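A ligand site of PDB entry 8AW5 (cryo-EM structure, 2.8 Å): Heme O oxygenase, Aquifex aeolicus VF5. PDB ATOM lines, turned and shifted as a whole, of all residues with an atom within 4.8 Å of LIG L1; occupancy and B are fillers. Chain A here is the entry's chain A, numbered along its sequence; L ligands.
A ring nitrogen (NE2) of His 266 binds an iron atom (FE1) of LIG L1, at 2.5 Å.
NE2 of His 213 binds FE1 of LIG L1, 2.5 Å away.
The guanidinium group of Arg 198 lies within salt-bridge range of an oxygen (O4) of LIG L1 (3.4 Å).
OH of Tyr 210 lies within hydrogen-bond range of O6 of LG2 L2 (2.7 Å).
The backbone carbonyl oxygen (O) of His 266 sits close to the side-chain amide oxygen (OE1) of Gln 246 (2.9 Å).
N of Gly 250 is in hydrogen-bond range of ND1 of His 266 (3.4 Å).
The side-chain amide oxygen of Gln 190 lies within hydrogen-bond range of a ring nitrogen (ND1) of His 213, 3.1 Å away.
NE2 of Gln 246 lies close to N of Gly 270 (3.4 Å).
NH2 of Arg 198 is in hydrogen-bond range of O of Gly 30 (3.0 Å).
N of Ala 217 lies close to NE2 of Gln 190 (3.5 Å).
Leu 149 touches LIG L1 (CD2 to O3, 3.2 Å).
NE2 of Gln 190 touches C21 of LIG L1, 3.3 Å away.
CD1 of Ile 191 touches C31 of LIG L1, at 3.4 Å.
Gly 194 touches LIG L1.
Val 197 touches LIG L1 (CG1 to C10, 3.7 Å).
CG2 of Ile 214 touches C17 of LIG L1, at 3.6 Å.
Ala 217 touches LIG L1 (CB to C19, 3.3 Å).
CD1 of Leu 220 touches C26 of LIG L1, 3.7 Å away.
SD of Met 243 touches C26 of LIG L1, at 3.9 Å.
Gln 246 touches LIG L1.
Ile 247 touches LIG L1.
C of Gly 250 touches C17 of LIG L1, 3.5 Å away.
N of Val 251 touches C17 of LIG L1, at 3.5 Å.
Val 254 touches LIG L1.
CE2 of Phe 258 touches O1 of LIG L1, at 3.4 Å.
Leu 263 touches LIG L1 (CD1 to O2, 3.3 Å).
Ile 267 touches LIG L1.
CZ of Phe 271 touches O4 of LIG L1, at 3.8 Å.
Ile 273 touches LIG L1 (CD1 to C26, 3.9 Å).
The nearest printed residue that does not touch LIG L1 is Ile 195 (4.02 Å).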
ATOM      1  N   GLY A  30     -18.492 -37.913 -15.587  1.00  0.00           N
ATOM      2  CA  GLY A  30     -19.317 -36.747 -15.839  1.00  0.00           C
ATOM      3  C   GLY A  30     -20.580 -36.669 -15.007  1.00  0.00           C
ATOM      4  O   GLY A  30     -21.261 -35.634 -14.983  1.00  0.00           O
ATOM      5  N   LEU A  52     -23.786 -21.631 -15.382  1.00  0.00           N
ATOM      6  CA  LEU A  52     -22.634 -21.109 -16.086  1.00  0.00           C
ATOM      7  C   LEU A  52     -22.221 -19.775 -15.472  1.00  0.00           C
ATOM      8  O   LEU A  52     -23.063 -19.002 -15.004  1.00  0.00           O
ATOM      9  CB  LEU A  52     -22.935 -20.949 -17.569  1.00  0.00           C
ATOM     10  CG  LEU A  52     -23.229 -22.268 -18.278  1.00  0.00           C
ATOM     11  CD1 LEU A  52     -23.503 -22.048 -19.746  1.00  0.00           C
ATOM     12  CD2 LEU A  52     -22.080 -23.246 -18.091  1.00  0.00           C
ATOM     13  N   LEU A 149     -10.748 -34.378 -20.407  1.00  0.00           N
ATOM     14  CA  LEU A 149     -11.914 -34.808 -21.175  1.00  0.00           C
ATOM     15  C   LEU A 149     -11.595 -34.977 -22.651  1.00  0.00           C
ATOM     16  O   LEU A 149     -12.149 -35.866 -23.299  1.00  0.00           O
ATOM     17  CB  LEU A 149     -13.058 -33.804 -20.993  1.00  0.00           C
ATOM     18  CG  LEU A 149     -14.416 -34.341 -21.431  1.00  0.00           C
ATOM     19  CD1 LEU A 149     -14.516 -35.816 -21.142  1.00  0.00           C
ATOM     20  CD2 LEU A 149     -15.516 -33.575 -20.727  1.00  0.00           C
ATOM     21  N   GLN A 190     -18.159 -30.088 -32.059  1.00  0.00           N
ATOM     22  CA  GLN A 190     -19.236 -29.800 -31.109  1.00  0.00           C
ATOM     23  C   GLN A 190     -18.933 -30.365 -29.722  1.00  0.00           C
ATOM     24  O   GLN A 190     -19.239 -29.734 -28.711  1.00  0.00           O
ATOM     25  CB  GLN A 190     -20.563 -30.348 -31.644  1.00  0.00           C
ATOM     26  CG  GLN A 190     -21.758 -30.102 -30.727  1.00  0.00           C
ATOM     27  CD  GLN A 190     -22.240 -28.667 -30.742  1.00  0.00           C
ATOM     28  OE1 GLN A 190     -21.504 -27.745 -31.084  1.00  0.00           O
ATOM     29  NE2 GLN A 190     -23.488 -28.466 -30.351  1.00  0.00           N
ATOM     30  N   ILE A 191     -18.349 -31.563 -29.671  1.00  0.00           N
ATOM     31  CA  ILE A 191     -17.963 -32.138 -28.388  1.00  0.00           C
ATOM     32  C   ILE A 191     -16.911 -31.277 -27.708  1.00  0.00           C
ATOM     33  O   ILE A 191     -16.933 -31.065 -26.497  1.00  0.00           O
ATOM     34  CB  ILE A 191     -17.476 -33.591 -28.581  1.00  0.00           C
ATOM     35  CG1 ILE A 191     -18.627 -34.479 -29.053  1.00  0.00           C
ATOM     36  CG2 ILE A 191     -16.899 -34.131 -27.290  1.00  0.00           C
ATOM     37  CD1 ILE A 191     -19.696 -34.699 -28.026  1.00  0.00           C
ATOM     38  N   GLY A 194     -18.622 -28.359 -26.206  1.00  0.00           N
ATOM     39  CA  GLY A 194     -19.276 -28.730 -24.969  1.00  0.00           C
ATOM     40  C   GLY A 194     -18.313 -28.870 -23.814  1.00  0.00           C
ATOM     41  O   GLY A 194     -18.602 -28.450 -22.692  1.00  0.00           O
ATOM     42  N   ILE A 195     -17.148 -29.460 -24.075  1.00  0.00           N
ATOM     43  CA  ILE A 195     -16.122 -29.587 -23.036  1.00  0.00           C
ATOM     44  C   ILE A 195     -15.662 -28.206 -22.588  1.00  0.00           C
ATOM     45  O   ILE A 195     -15.486 -27.957 -21.384  1.00  0.00           O
ATOM     46  CB  ILE A 195     -14.937 -30.433 -23.550  1.00  0.00           C
ATOM     47  CG1 ILE A 195     -15.400 -31.861 -23.840  1.00  0.00           C
ATOM     48  CG2 ILE A 195     -13.805 -30.438 -22.544  1.00  0.00           C
ATOM     49  CD1 ILE A 195     -14.413 -32.659 -24.656  1.00  0.00           C
ATOM     50  N   VAL A 197     -17.402 -25.420 -22.692  1.00  0.00           N
ATOM     51  CA  VAL A 197     -18.484 -24.843 -21.899  1.00  0.00           C
ATOM     52  C   VAL A 197     -18.460 -25.412 -20.480  1.00  0.00           C
ATOM     53  O   VAL A 197     -18.621 -24.684 -19.499  1.00  0.00           O
ATOM     54  CB  VAL A 197     -19.841 -25.088 -22.582  1.00  0.00           C
ATOM     55  CG1 VAL A 197     -20.969 -24.622 -21.687  1.00  0.00           C
ATOM     56  CG2 VAL A 197     -19.903 -24.385 -23.913  1.00  0.00           C
ATOM     57  N   ARG A 198     -18.265 -26.728 -20.372  1.00  0.00           N
ATOM     58  CA  ARG A 198     -18.299 -27.371 -19.071  1.00  0.00           C
ATOM     59  C   ARG A 198     -17.156 -26.914 -18.179  1.00  0.00           C
ATOM     60  O   ARG A 198     -17.355 -26.652 -16.987  1.00  0.00           O
ATOM     61  CB  ARG A 198     -18.256 -28.892 -19.264  1.00  0.00           C
ATOM     62  CG  ARG A 198     -18.066 -29.696 -17.998  1.00  0.00           C
ATOM     63  CD  ARG A 198     -19.273 -30.524 -17.650  1.00  0.00           C
ATOM     64  NE  ARG A 198     -18.992 -31.431 -16.550  1.00  0.00           N
ATOM     65  CZ  ARG A 198     -19.732 -32.501 -16.260  1.00  0.00           C
ATOM     66  NH1 ARG A 198     -20.849 -32.732 -16.934  1.00  0.00           N
ATOM     67  NH2 ARG A 198     -19.348 -33.337 -15.313  1.00  0.00           N
ATOM     68  N   TYR A 199     -15.938 -26.811 -18.730  1.00  0.00           N
ATOM     69  CA  TYR A 199     -14.763 -26.661 -17.899  1.00  0.00           C
ATOM     70  C   TYR A 199     -14.080 -25.301 -17.974  1.00  0.00           C
ATOM     71  O   TYR A 199     -13.578 -24.824 -16.957  1.00  0.00           O
ATOM     72  CB  TYR A 199     -13.741 -27.751 -18.226  1.00  0.00           C
ATOM     73  CG  TYR A 199     -14.228 -29.130 -17.864  1.00  0.00           C
ATOM     74  CD1 TYR A 199     -14.859 -29.346 -16.648  1.00  0.00           C
ATOM     75  CD2 TYR A 199     -14.084 -30.196 -18.726  1.00  0.00           C
ATOM     76  CE1 TYR A 199     -15.324 -30.599 -16.306  1.00  0.00           C
ATOM     77  CE2 TYR A 199     -14.542 -31.447 -18.400  1.00  0.00           C
ATOM     78  CZ  TYR A 199     -15.167 -31.647 -17.186  1.00  0.00           C
ATOM     79  OH  TYR A 199     -15.624 -32.891 -16.838  1.00  0.00           O
ATOM     80  N   TYR A 210     -20.457 -20.969 -24.907  1.00  0.00           N
ATOM     81  CA  TYR A 210     -21.796 -21.502 -24.713  1.00  0.00           C
ATOM     82  C   TYR A 210     -22.726 -21.079 -25.844  1.00  0.00           C
ATOM     83  O   TYR A 210     -23.484 -21.905 -26.387  1.00  0.00           O
ATOM     84  CB  TYR A 210     -22.346 -21.053 -23.363  1.00  0.00           C
ATOM     85  CG  TYR A 210     -23.840 -21.204 -23.214  1.00  0.00           C
ATOM     86  CD1 TYR A 210     -24.424 -22.452 -23.163  1.00  0.00           C
ATOM     87  CD2 TYR A 210     -24.652 -20.091 -23.131  1.00  0.00           C
ATOM     88  CE1 TYR A 210     -25.787 -22.593 -23.033  1.00  0.00           C
ATOM     89  CE2 TYR A 210     -26.010 -20.215 -23.002  1.00  0.00           C
ATOM     90  CZ  TYR A 210     -26.571 -21.471 -22.954  1.00  0.00           C
ATOM     91  OH  TYR A 210     -27.931 -21.589 -22.832  1.00  0.00           O
ATOM     92  N   HIS A 213     -21.748 -23.021 -28.864  1.00  0.00           N
ATOM     93  CA  HIS A 213     -22.205 -24.409 -28.741  1.00  0.00           C
ATOM     94  C   HIS A 213     -23.670 -24.536 -29.133  1.00  0.00           C
ATOM     95  O   HIS A 213     -24.039 -25.366 -29.980  1.00  0.00           O
ATOM     96  CB  HIS A 213     -21.966 -24.876 -27.304  1.00  0.00           C
ATOM     97  CG  HIS A 213     -22.072 -26.351 -27.128  1.00  0.00           C
ATOM     98  ND1 HIS A 213     -21.483 -27.253 -28.000  1.00  0.00           N
ATOM     99  CD2 HIS A 213     -22.665 -27.091 -26.168  1.00  0.00           C
ATOM    100  CE1 HIS A 213     -21.724 -28.477 -27.583  1.00  0.00           C
ATOM    101  NE2 HIS A 213     -22.433 -28.420 -26.479  1.00  0.00           N
ATOM    102  N   ILE A 214     -24.525 -23.717 -28.514  1.00  0.00           N
ATOM    103  CA  ILE A 214     -25.985 -23.800 -28.779  1.00  0.00           C
ATOM    104  C   ILE A 214     -26.268 -23.479 -30.248  1.00  0.00           C
ATOM    105  O   ILE A 214     -27.248 -24.025 -30.789  1.00  0.00           O
ATOM    106  CB  ILE A 214     -26.779 -22.879 -27.829  1.00  0.00           C
ATOM    107  CG1 ILE A 214     -26.426 -21.402 -28.040  1.00  0.00           C
ATOM    108  CG2 ILE A 214     -26.565 -23.294 -26.376  1.00  0.00           C
ATOM    109  CD1 ILE A 214     -26.834 -20.509 -26.893  1.00  0.00           C
ATOM    110  N   ALA A 217     -25.017 -26.367 -32.652  1.00  0.00           N
ATOM    111  CA  ALA A 217     -25.983 -27.457 -32.644  1.00  0.00           C
ATOM    112  C   ALA A 217     -26.912 -27.379 -33.845  1.00  0.00           C
ATOM    113  O   ALA A 217     -27.305 -28.406 -34.405  1.00  0.00           O
ATOM    114  CB  ALA A 217     -26.784 -27.415 -31.341  1.00  0.00           C
ATOM    115  N   LEU A 220     -25.148 -28.812 -36.781  1.00  0.00           N
ATOM    116  CA  LEU A 220     -25.177 -30.270 -36.694  1.00  0.00           C
ATOM    117  C   LEU A 220     -26.518 -30.831 -37.135  1.00  0.00           C
ATOM    118  O   LEU A 220     -26.586 -31.845 -37.826  1.00  0.00           O
ATOM    119  CB  LEU A 220     -24.828 -30.732 -35.288  1.00  0.00           C
ATOM    120  CG  LEU A 220     -23.349 -30.910 -35.004  1.00  0.00           C
ATOM    121  CD1 LEU A 220     -23.153 -31.653 -33.711  1.00  0.00           C
ATOM    122  CD2 LEU A 220     -22.683 -31.645 -36.155  1.00  0.00           C
ATOM    123  N   MET A 243     -28.942 -36.515 -32.535  1.00  0.00           N
ATOM    124  CA  MET A 243     -28.706 -35.085 -32.492  1.00  0.00           C
ATOM    125  C   MET A 243     -29.902 -34.453 -31.785  1.00  0.00           C
ATOM    126  O   MET A 243     -29.745 -33.830 -30.724  1.00  0.00           O
ATOM    127  CB  MET A 243     -28.424 -34.543 -33.896  1.00  0.00           C
ATOM    128  CG  MET A 243     -27.148 -35.086 -34.524  1.00  0.00           C
ATOM    129  SD  MET A 243     -25.682 -34.687 -33.568  1.00  0.00           S
ATOM    130  CE  MET A 243     -24.422 -35.489 -34.551  1.00  0.00           C
ATOM    131  N   GLN A 246     -30.043 -35.038 -28.093  1.00  0.00           N
ATOM    132  CA  GLN A 246     -29.015 -34.288 -27.378  1.00  0.00           C
ATOM    133  C   GLN A 246     -29.327 -32.803 -27.289  1.00  0.00           C
ATOM    134  O   GLN A 246     -29.011 -32.146 -26.294  1.00  0.00           O
ATOM    135  CB  GLN A 246     -27.662 -34.489 -28.062  1.00  0.00           C
ATOM    136  CG  GLN A 246     -26.527 -33.713 -27.427  1.00  0.00           C
ATOM    137  CD  GLN A 246     -26.073 -34.275 -26.090  1.00  0.00           C
ATOM    138  OE1 GLN A 246     -26.834 -34.937 -25.387  1.00  0.00           O
ATOM    139  NE2 GLN A 246     -24.827 -34.000 -25.736  1.00  0.00           N
ATOM    140  N   ILE A 247     -29.855 -32.244 -28.352  1.00  0.00           N
ATOM    141  CA  ILE A 247     -30.182 -30.783 -28.410  1.00  0.00           C
ATOM    142  C   ILE A 247     -31.293 -30.617 -27.374  1.00  0.00           C
ATOM    143  O   ILE A 247     -31.082 -29.867 -26.402  1.00  0.00           O
ATOM    144  CB  ILE A 247     -30.502 -30.327 -29.849  1.00  0.00           C
ATOM    145  CG1 ILE A 247     -31.904 -30.721 -30.293  1.00  0.00           C
ATOM    146  CG2 ILE A 247     -29.448 -30.828 -30.819  1.00  0.00           C
ATOM    147  CD1 ILE A 247     -32.239 -30.313 -31.714  1.00  0.00           C
ATOM    148  N   GLY A 250     -29.913 -30.851 -23.953  1.00  0.00           N
ATOM    149  CA  GLY A 250     -29.128 -29.643 -23.653  1.00  0.00           C
ATOM    150  C   GLY A 250     -30.026 -28.486 -23.273  1.00  0.00           C
ATOM    151  O   GLY A 250     -29.775 -27.865 -22.226  1.00  0.00           O
ATOM    152  N   VAL A 251     -31.036 -28.203 -24.097  1.00  0.00           N
ATOM    153  CA  VAL A 251     -31.980 -27.081 -23.817  1.00  0.00           C
ATOM    154  C   VAL A 251     -32.605 -27.306 -22.438  1.00  0.00           C
ATOM    155  O   VAL A 251     -32.542 -26.383 -21.615  1.00  0.00           O
ATOM    156  CB  VAL A 251     -33.070 -26.980 -24.910  1.00  0.00           C
ATOM    157  CG1 VAL A 251     -33.897 -25.718 -24.765  1.00  0.00           C
ATOM    158  CG2 VAL A 251     -32.464 -27.079 -26.299  1.00  0.00           C
ATOM    159  N   VAL A 254     -30.693 -26.430 -19.629  1.00  0.00           N
ATOM    160  CA  VAL A 254     -30.708 -24.937 -19.518  1.00  0.00           C
ATOM    161  C   VAL A 254     -32.088 -24.340 -19.198  1.00  0.00           C
ATOM    162  O   VAL A 254     -32.132 -23.307 -18.513  1.00  0.00           O
ATOM    163  CB  VAL A 254     -30.114 -24.325 -20.803  1.00  0.00           C
ATOM    164  CG1 VAL A 254     -29.894 -22.827 -20.660  1.00  0.00           C
ATOM    165  CG2 VAL A 254     -28.834 -25.018 -21.213  1.00  0.00           C
ATOM    166  N   PHE A 258     -29.927 -26.299 -13.476  1.00  0.00           N
ATOM    167  CA  PHE A 258     -29.003 -27.373 -13.933  1.00  0.00           C
ATOM    168  C   PHE A 258     -29.422 -28.691 -13.267  1.00  0.00           C
ATOM    169  O   PHE A 258     -28.604 -29.297 -12.551  1.00  0.00           O
ATOM    170  CB  PHE A 258     -27.553 -27.006 -13.581  1.00  0.00           C
ATOM    171  CG  PHE A 258     -26.773 -26.370 -14.707  1.00  0.00           C
ATOM    172  CD1 PHE A 258     -27.189 -25.172 -15.268  1.00  0.00           C
ATOM    173  CD2 PHE A 258     -25.629 -26.970 -15.201  1.00  0.00           C
ATOM    174  CE1 PHE A 258     -26.474 -24.593 -16.305  1.00  0.00           C
ATOM    175  CE2 PHE A 258     -24.915 -26.384 -16.231  1.00  0.00           C
ATOM    176  CZ  PHE A 258     -25.337 -25.195 -16.783  1.00  0.00           C
ATOM    177  N   LEU A 263     -28.888 -32.902 -16.749  1.00  0.00           N
ATOM    178  CA  LEU A 263     -27.435 -32.726 -16.985  1.00  0.00           C
ATOM    179  C   LEU A 263     -26.785 -34.076 -17.296  1.00  0.00           C
ATOM    180  O   LEU A 263     -25.888 -34.117 -18.163  1.00  0.00           O
ATOM    181  CB  LEU A 263     -26.797 -32.131 -15.726  1.00  0.00           C
ATOM    182  CG  LEU A 263     -25.295 -31.898 -15.800  1.00  0.00           C
ATOM    183  CD1 LEU A 263     -24.917 -31.210 -17.107  1.00  0.00           C
ATOM    184  CD2 LEU A 263     -24.808 -31.082 -14.611  1.00  0.00           C
ATOM    185  N   HIS A 266     -27.829 -35.573 -20.788  1.00  0.00           N
ATOM    186  CA  HIS A 266     -27.098 -34.820 -21.796  1.00  0.00           C
ATOM    187  C   HIS A 266     -25.675 -35.370 -21.944  1.00  0.00           C
ATOM    188  O   HIS A 266     -25.197 -35.578 -23.063  1.00  0.00           O
ATOM    189  CB  HIS A 266     -27.078 -33.349 -21.418  1.00  0.00           C
ATOM    190  CG  HIS A 266     -26.417 -32.470 -22.420  1.00  0.00           C
ATOM    191  ND1 HIS A 266     -26.862 -32.333 -23.718  1.00  0.00           N
ATOM    192  CD2 HIS A 266     -25.323 -31.682 -22.322  1.00  0.00           C
ATOM    193  CE1 HIS A 266     -26.082 -31.497 -24.364  1.00  0.00           C
ATOM    194  NE2 HIS A 266     -25.137 -31.083 -23.543  1.00  0.00           N
ATOM    195  N   ILE A 267     -25.002 -35.612 -20.818  1.00  0.00           N
ATOM    196  CA  ILE A 267     -23.632 -36.143 -20.852  1.00  0.00           C
ATOM    197  C   ILE A 267     -23.616 -37.518 -21.503  1.00  0.00           C
ATOM    198  O   ILE A 267     -22.772 -37.826 -22.355  1.00  0.00           O
ATOM    199  CB  ILE A 267     -23.051 -36.181 -19.432  1.00  0.00           C
ATOM    200  CG1 ILE A 267     -23.076 -34.787 -18.802  1.00  0.00           C
ATOM    201  CG2 ILE A 267     -21.645 -36.746 -19.442  1.00  0.00           C
ATOM    202  CD1 ILE A 267     -23.251 -34.804 -17.306  1.00  0.00           C
ATOM    203  N   GLY A 270     -24.229 -37.277 -25.223  1.00  0.00           N
ATOM    204  CA  GLY A 270     -23.090 -36.709 -25.919  1.00  0.00           C
ATOM    205  C   GLY A 270     -21.967 -37.718 -26.113  1.00  0.00           C
ATOM    206  O   GLY A 270     -21.398 -37.833 -27.211  1.00  0.00           O
ATOM    207  N   PHE A 271     -21.648 -38.465 -25.066  1.00  0.00           N
ATOM    208  CA  PHE A 271     -20.578 -39.455 -25.217  1.00  0.00           C
ATOM    209  C   PHE A 271     -21.004 -40.604 -26.112  1.00  0.00           C
ATOM    210  O   PHE A 271     -20.181 -41.149 -26.876  1.00  0.00           O
ATOM    211  CB  PHE A 271     -20.119 -39.950 -23.846  1.00  0.00           C
ATOM    212  CG  PHE A 271     -19.346 -38.923 -23.075  1.00  0.00           C
ATOM    213  CD1 PHE A 271     -18.662 -37.916 -23.734  1.00  0.00           C
ATOM    214  CD2 PHE A 271     -19.300 -38.959 -21.695  1.00  0.00           C
ATOM    215  CE1 PHE A 271     -17.951 -36.965 -23.037  1.00  0.00           C
ATOM    216  CE2 PHE A 271     -18.585 -38.015 -20.992  1.00  0.00           C
ATOM    217  CZ  PHE A 271     -17.912 -37.018 -21.670  1.00  0.00           C
ATOM    218  N   ILE A 273     -22.966 -40.190 -28.670  1.00  0.00           N
ATOM    219  CA  ILE A 273     -22.782 -39.591 -29.976  1.00  0.00           C
ATOM    220  C   ILE A 273     -21.346 -39.645 -30.440  1.00  0.00           C
ATOM    221  O   ILE A 273     -21.063 -39.896 -31.615  1.00  0.00           O
ATOM    222  CB  ILE A 273     -23.337 -38.155 -29.988  1.00  0.00           C
ATOM    223  CG1 ILE A 273     -24.870 -38.175 -29.973  1.00  0.00           C
ATOM    224  CG2 ILE A 273     -22.859 -37.402 -31.204  1.00  0.00           C
ATOM    225  CD1 ILE A 273     -25.480 -36.802 -29.918  1.00  0.00           C
HETATM  226  C1  LIG L   1     -22.182 -29.403 -22.380  1.00  0.00           C
HETATM  227  C2  LIG L   1     -26.285 -27.031 -23.321  1.00  0.00           C
HETATM  228  C3  LIG L   1     -26.430 -28.988 -27.762  1.00  0.00           C
HETATM  229  C4  LIG L   1     -22.716 -31.851 -26.525  1.00  0.00           C
HETATM  230  C5  LIG L   1     -23.250 -28.545 -22.269  1.00  0.00           C
HETATM  231  C6  LIG L   1     -23.502 -27.641 -21.180  1.00  0.00           C
HETATM  232  C7  LIG L   1     -24.626 -26.986 -21.440  1.00  0.00           C
HETATM  233  C8  LIG L   1     -25.136 -27.454 -22.706  1.00  0.00           C
HETATM  234  C9  LIG L   1     -25.285 -25.913 -20.549  1.00  0.00           C
HETATM  235  C10 LIG L   1     -22.627 -27.440 -19.922  1.00  0.00           C
HETATM  236  C11 LIG L   1     -22.675 -28.715 -19.087  1.00  0.00           C
HETATM  237  C12 LIG L   1     -22.178 -28.423 -17.694  1.00  0.00           C
HETATM  238  O1  LIG L   1     -21.806 -27.259 -17.427  1.00  0.00           O
HETATM  239  O2  LIG L   1     -22.169 -29.357 -16.848  1.00  0.00           O
HETATM  240  C13 LIG L   1     -26.665 -27.311 -24.611  1.00  0.00           C
HETATM  241  C14 LIG L   1     -27.776 -26.705 -25.315  1.00  0.00           C
HETATM  242  C15 LIG L   1     -27.821 -27.225 -26.544  1.00  0.00           C
HETATM  243  C16 LIG L   1     -26.751 -28.200 -26.667  1.00  0.00           C
HETATM  244  C17 LIG L   1     -28.725 -25.641 -24.754  1.00  0.00           C
HETATM  245  C18 LIG L   1     -28.895 -26.795 -27.563  1.00  0.00           C
HETATM  246  C19 LIG L   1     -28.953 -27.304 -28.791  1.00  0.00           C
HETATM  247  C20 LIG L   1     -25.453 -29.963 -27.800  1.00  0.00           C
HETATM  248  C21 LIG L   1     -25.198 -30.881 -28.890  1.00  0.00           C
HETATM  249  C22 LIG L   1     -24.158 -31.665 -28.542  1.00  0.00           C
HETATM  250  C23 LIG L   1     -23.744 -31.272 -27.218  1.00  0.00           C
HETATM  251  C24 LIG L   1     -25.999 -30.904 -30.213  1.00  0.00           C
HETATM  252  C25 LIG L   1     -23.463 -32.826 -29.301  1.00  0.00           C
HETATM  253  C26 LIG L   1     -23.816 -33.291 -30.503  1.00  0.00           C
HETATM  254  C27 LIG L   1     -22.253 -31.449 -25.286  1.00  0.00           C
HETATM  255  C28 LIG L   1     -21.167 -32.056 -24.543  1.00  0.00           C
HETATM  256  C29 LIG L   1     -21.026 -31.380 -23.410  1.00  0.00           C
HETATM  257  C30 LIG L   1     -22.010 -30.319 -23.386  1.00  0.00           C
HETATM  258  C31 LIG L   1     -20.335 -33.275 -24.997  1.00  0.00           C
HETATM  259  C32 LIG L   1     -19.992 -31.668 -22.296  1.00  0.00           C
HETATM  260  C33 LIG L   1     -20.488 -32.792 -21.396  1.00  0.00           C
HETATM  261  C34 LIG L   1     -19.395 -33.134 -20.419  1.00  0.00           C
HETATM  262  O3  LIG L   1     -18.403 -32.363 -20.335  1.00  0.00           O
HETATM  263  O4  LIG L   1     -19.514 -34.170 -19.717  1.00  0.00           O
HETATM  264  N1  LIG L   1     -24.262 -28.409 -23.188  1.00  0.00           N
HETATM  265  N2  LIG L   1     -26.074 -28.213 -25.469  1.00  0.00           N
HETATM  266  N3  LIG L   1     -24.548 -30.229 -26.798  1.00  0.00           N
HETATM  267  N4  LIG L   1     -22.742 -30.389 -24.554  1.00  0.00           N
HETATM  268 FE1  LIG L   1     -24.373 -29.227 -25.050  1.00  0.00          FE
HETATM  269  N1  LG2 L   2     -32.408 -12.123 -19.064  1.00  0.00           N
HETATM  270  P1  LG2 L   2     -30.428 -14.700 -22.113  1.00  0.00           P
HETATM  271  C1  LG2 L   2     -28.940 -16.845 -22.534  1.00  0.00           C
HETATM  272  C2  LG2 L   2     -29.716 -17.819 -23.428  1.00  0.00           C
HETATM  273  C3  LG2 L   2     -29.911 -17.185 -24.796  1.00  0.00           C
HETATM  274  C4  LG2 L   2     -30.571 -23.935 -30.870  1.00  0.00           C
HETATM  275  C5  LG2 L   2     -36.245 -24.657 -33.886  1.00  0.00           C
HETATM  276  C6  LG2 L   2     -30.418 -13.343 -19.823  1.00  0.00           C
HETATM  277  O1  LG2 L   2     -29.263 -15.504 -22.883  1.00  0.00           O
HETATM  278  C7  LG2 L   2     -31.248 -25.043 -31.660  1.00  0.00           C
HETATM  279  C8  LG2 L   2     -37.330 -24.985 -34.897  1.00  0.00           C
HETATM  280  C9  LG2 L   2     -31.938 -13.239 -19.899  1.00  0.00           C
HETATM  281  O2  LG2 L   2     -29.967 -14.466 -20.584  1.00  0.00           O
HETATM  282  C10 LG2 L   2     -31.239 -24.686 -33.149  1.00  0.00           C
HETATM  283  C11 LG2 L   2     -37.145 -26.383 -35.456  1.00  0.00           C
HETATM  284  C12 LG2 L   2     -31.776 -10.870 -19.493  1.00  0.00           C
HETATM  285  O3  LG2 L   2     -30.629 -13.369 -22.800  1.00  0.00           O
HETATM  286  C13 LG2 L   2     -31.916 -25.756 -34.004  1.00  0.00           C
HETATM  287  C14 LG2 L   2     -38.101 -26.647 -36.608  1.00  0.00           C
HETATM  288  C15 LG2 L   2     -33.857 -11.998 -19.179  1.00  0.00           C
HETATM  289  O4  LG2 L   2     -31.707 -15.500 -22.127  1.00  0.00           O
HETATM  290  C16 LG2 L   2     -32.040 -25.248 -35.436  1.00  0.00           C
HETATM  291  C17 LG2 L   2     -39.557 -26.443 -36.182  1.00  0.00           C
HETATM  292  C18 LG2 L   2     -32.047 -12.383 -17.657  1.00  0.00           C
HETATM  293  C19 LG2 L   2     -32.471 -26.346 -36.396  1.00  0.00           C
HETATM  294  C20 LG2 L   2     -39.995 -27.492 -35.164  1.00  0.00           C
HETATM  295  C21 LG2 L   2     -32.450 -25.823 -37.820  1.00  0.00           C
HETATM  296  C22 LG2 L   2     -40.003 -28.874 -35.782  1.00  0.00           C
HETATM  297  C23 LG2 L   2     -32.681 -26.942 -38.829  1.00  0.00           C
HETATM  298  C24 LG2 L   2     -34.047 -27.564 -38.636  1.00  0.00           C
HETATM  299  C25 LG2 L   2     -31.147 -19.448 -22.469  1.00  0.00           C
HETATM  300  O5  LG2 L   2     -30.983 -18.085 -22.837  1.00  0.00           O
HETATM  301  C26 LG2 L   2     -31.506 -20.262 -23.711  1.00  0.00           C
HETATM  302  O6  LG2 L   2     -29.916 -19.934 -21.921  1.00  0.00           O
HETATM  303  C27 LG2 L   2     -31.987 -21.668 -23.363  1.00  0.00           C
HETATM  304  C28 LG2 L   2     -32.256 -22.447 -24.640  1.00  0.00           C
HETATM  305  C29 LG2 L   2     -30.966 -22.599 -25.438  1.00  0.00           C
HETATM  306  C30 LG2 L   2     -31.227 -22.537 -26.931  1.00  0.00           C
HETATM  307  C31 LG2 L   2     -32.157 -23.654 -27.385  1.00  0.00           C
HETATM  308  C32 LG2 L   2     -32.117 -23.796 -28.901  1.00  0.00           C
HETATM  309  C33 LG2 L   2     -30.718 -24.142 -29.366  1.00  0.00           C
HETATM  310  C34 LG2 L   2     -31.336 -18.011 -26.496  1.00  0.00           C
HETATM  311  O7  LG2 L   2     -30.107 -18.197 -25.777  1.00  0.00           O
HETATM  312  C35 LG2 L   2     -31.312 -18.849 -27.769  1.00  0.00           C
HETATM  313  O8  LG2 L   2     -31.487 -16.634 -26.827  1.00  0.00           O
HETATM  314  C36 LG2 L   2     -32.691 -18.894 -28.411  1.00  0.00           C
HETATM  315  C37 LG2 L   2     -32.658 -19.729 -29.686  1.00  0.00           C
HETATM  316  C38 LG2 L   2     -34.050 -20.024 -30.212  1.00  0.00           C
HETATM  317  C39 LG2 L   2     -33.957 -21.095 -31.289  1.00  0.00           C
HETATM  318  C40 LG2 L   2     -35.314 -21.541 -31.815  1.00  0.00           C
HETATM  319  C41 LG2 L   2     -35.146 -22.846 -32.582  1.00  0.00           C
HETATM  320  C42 LG2 L   2     -36.418 -23.256 -33.314  1.00  0.00           C
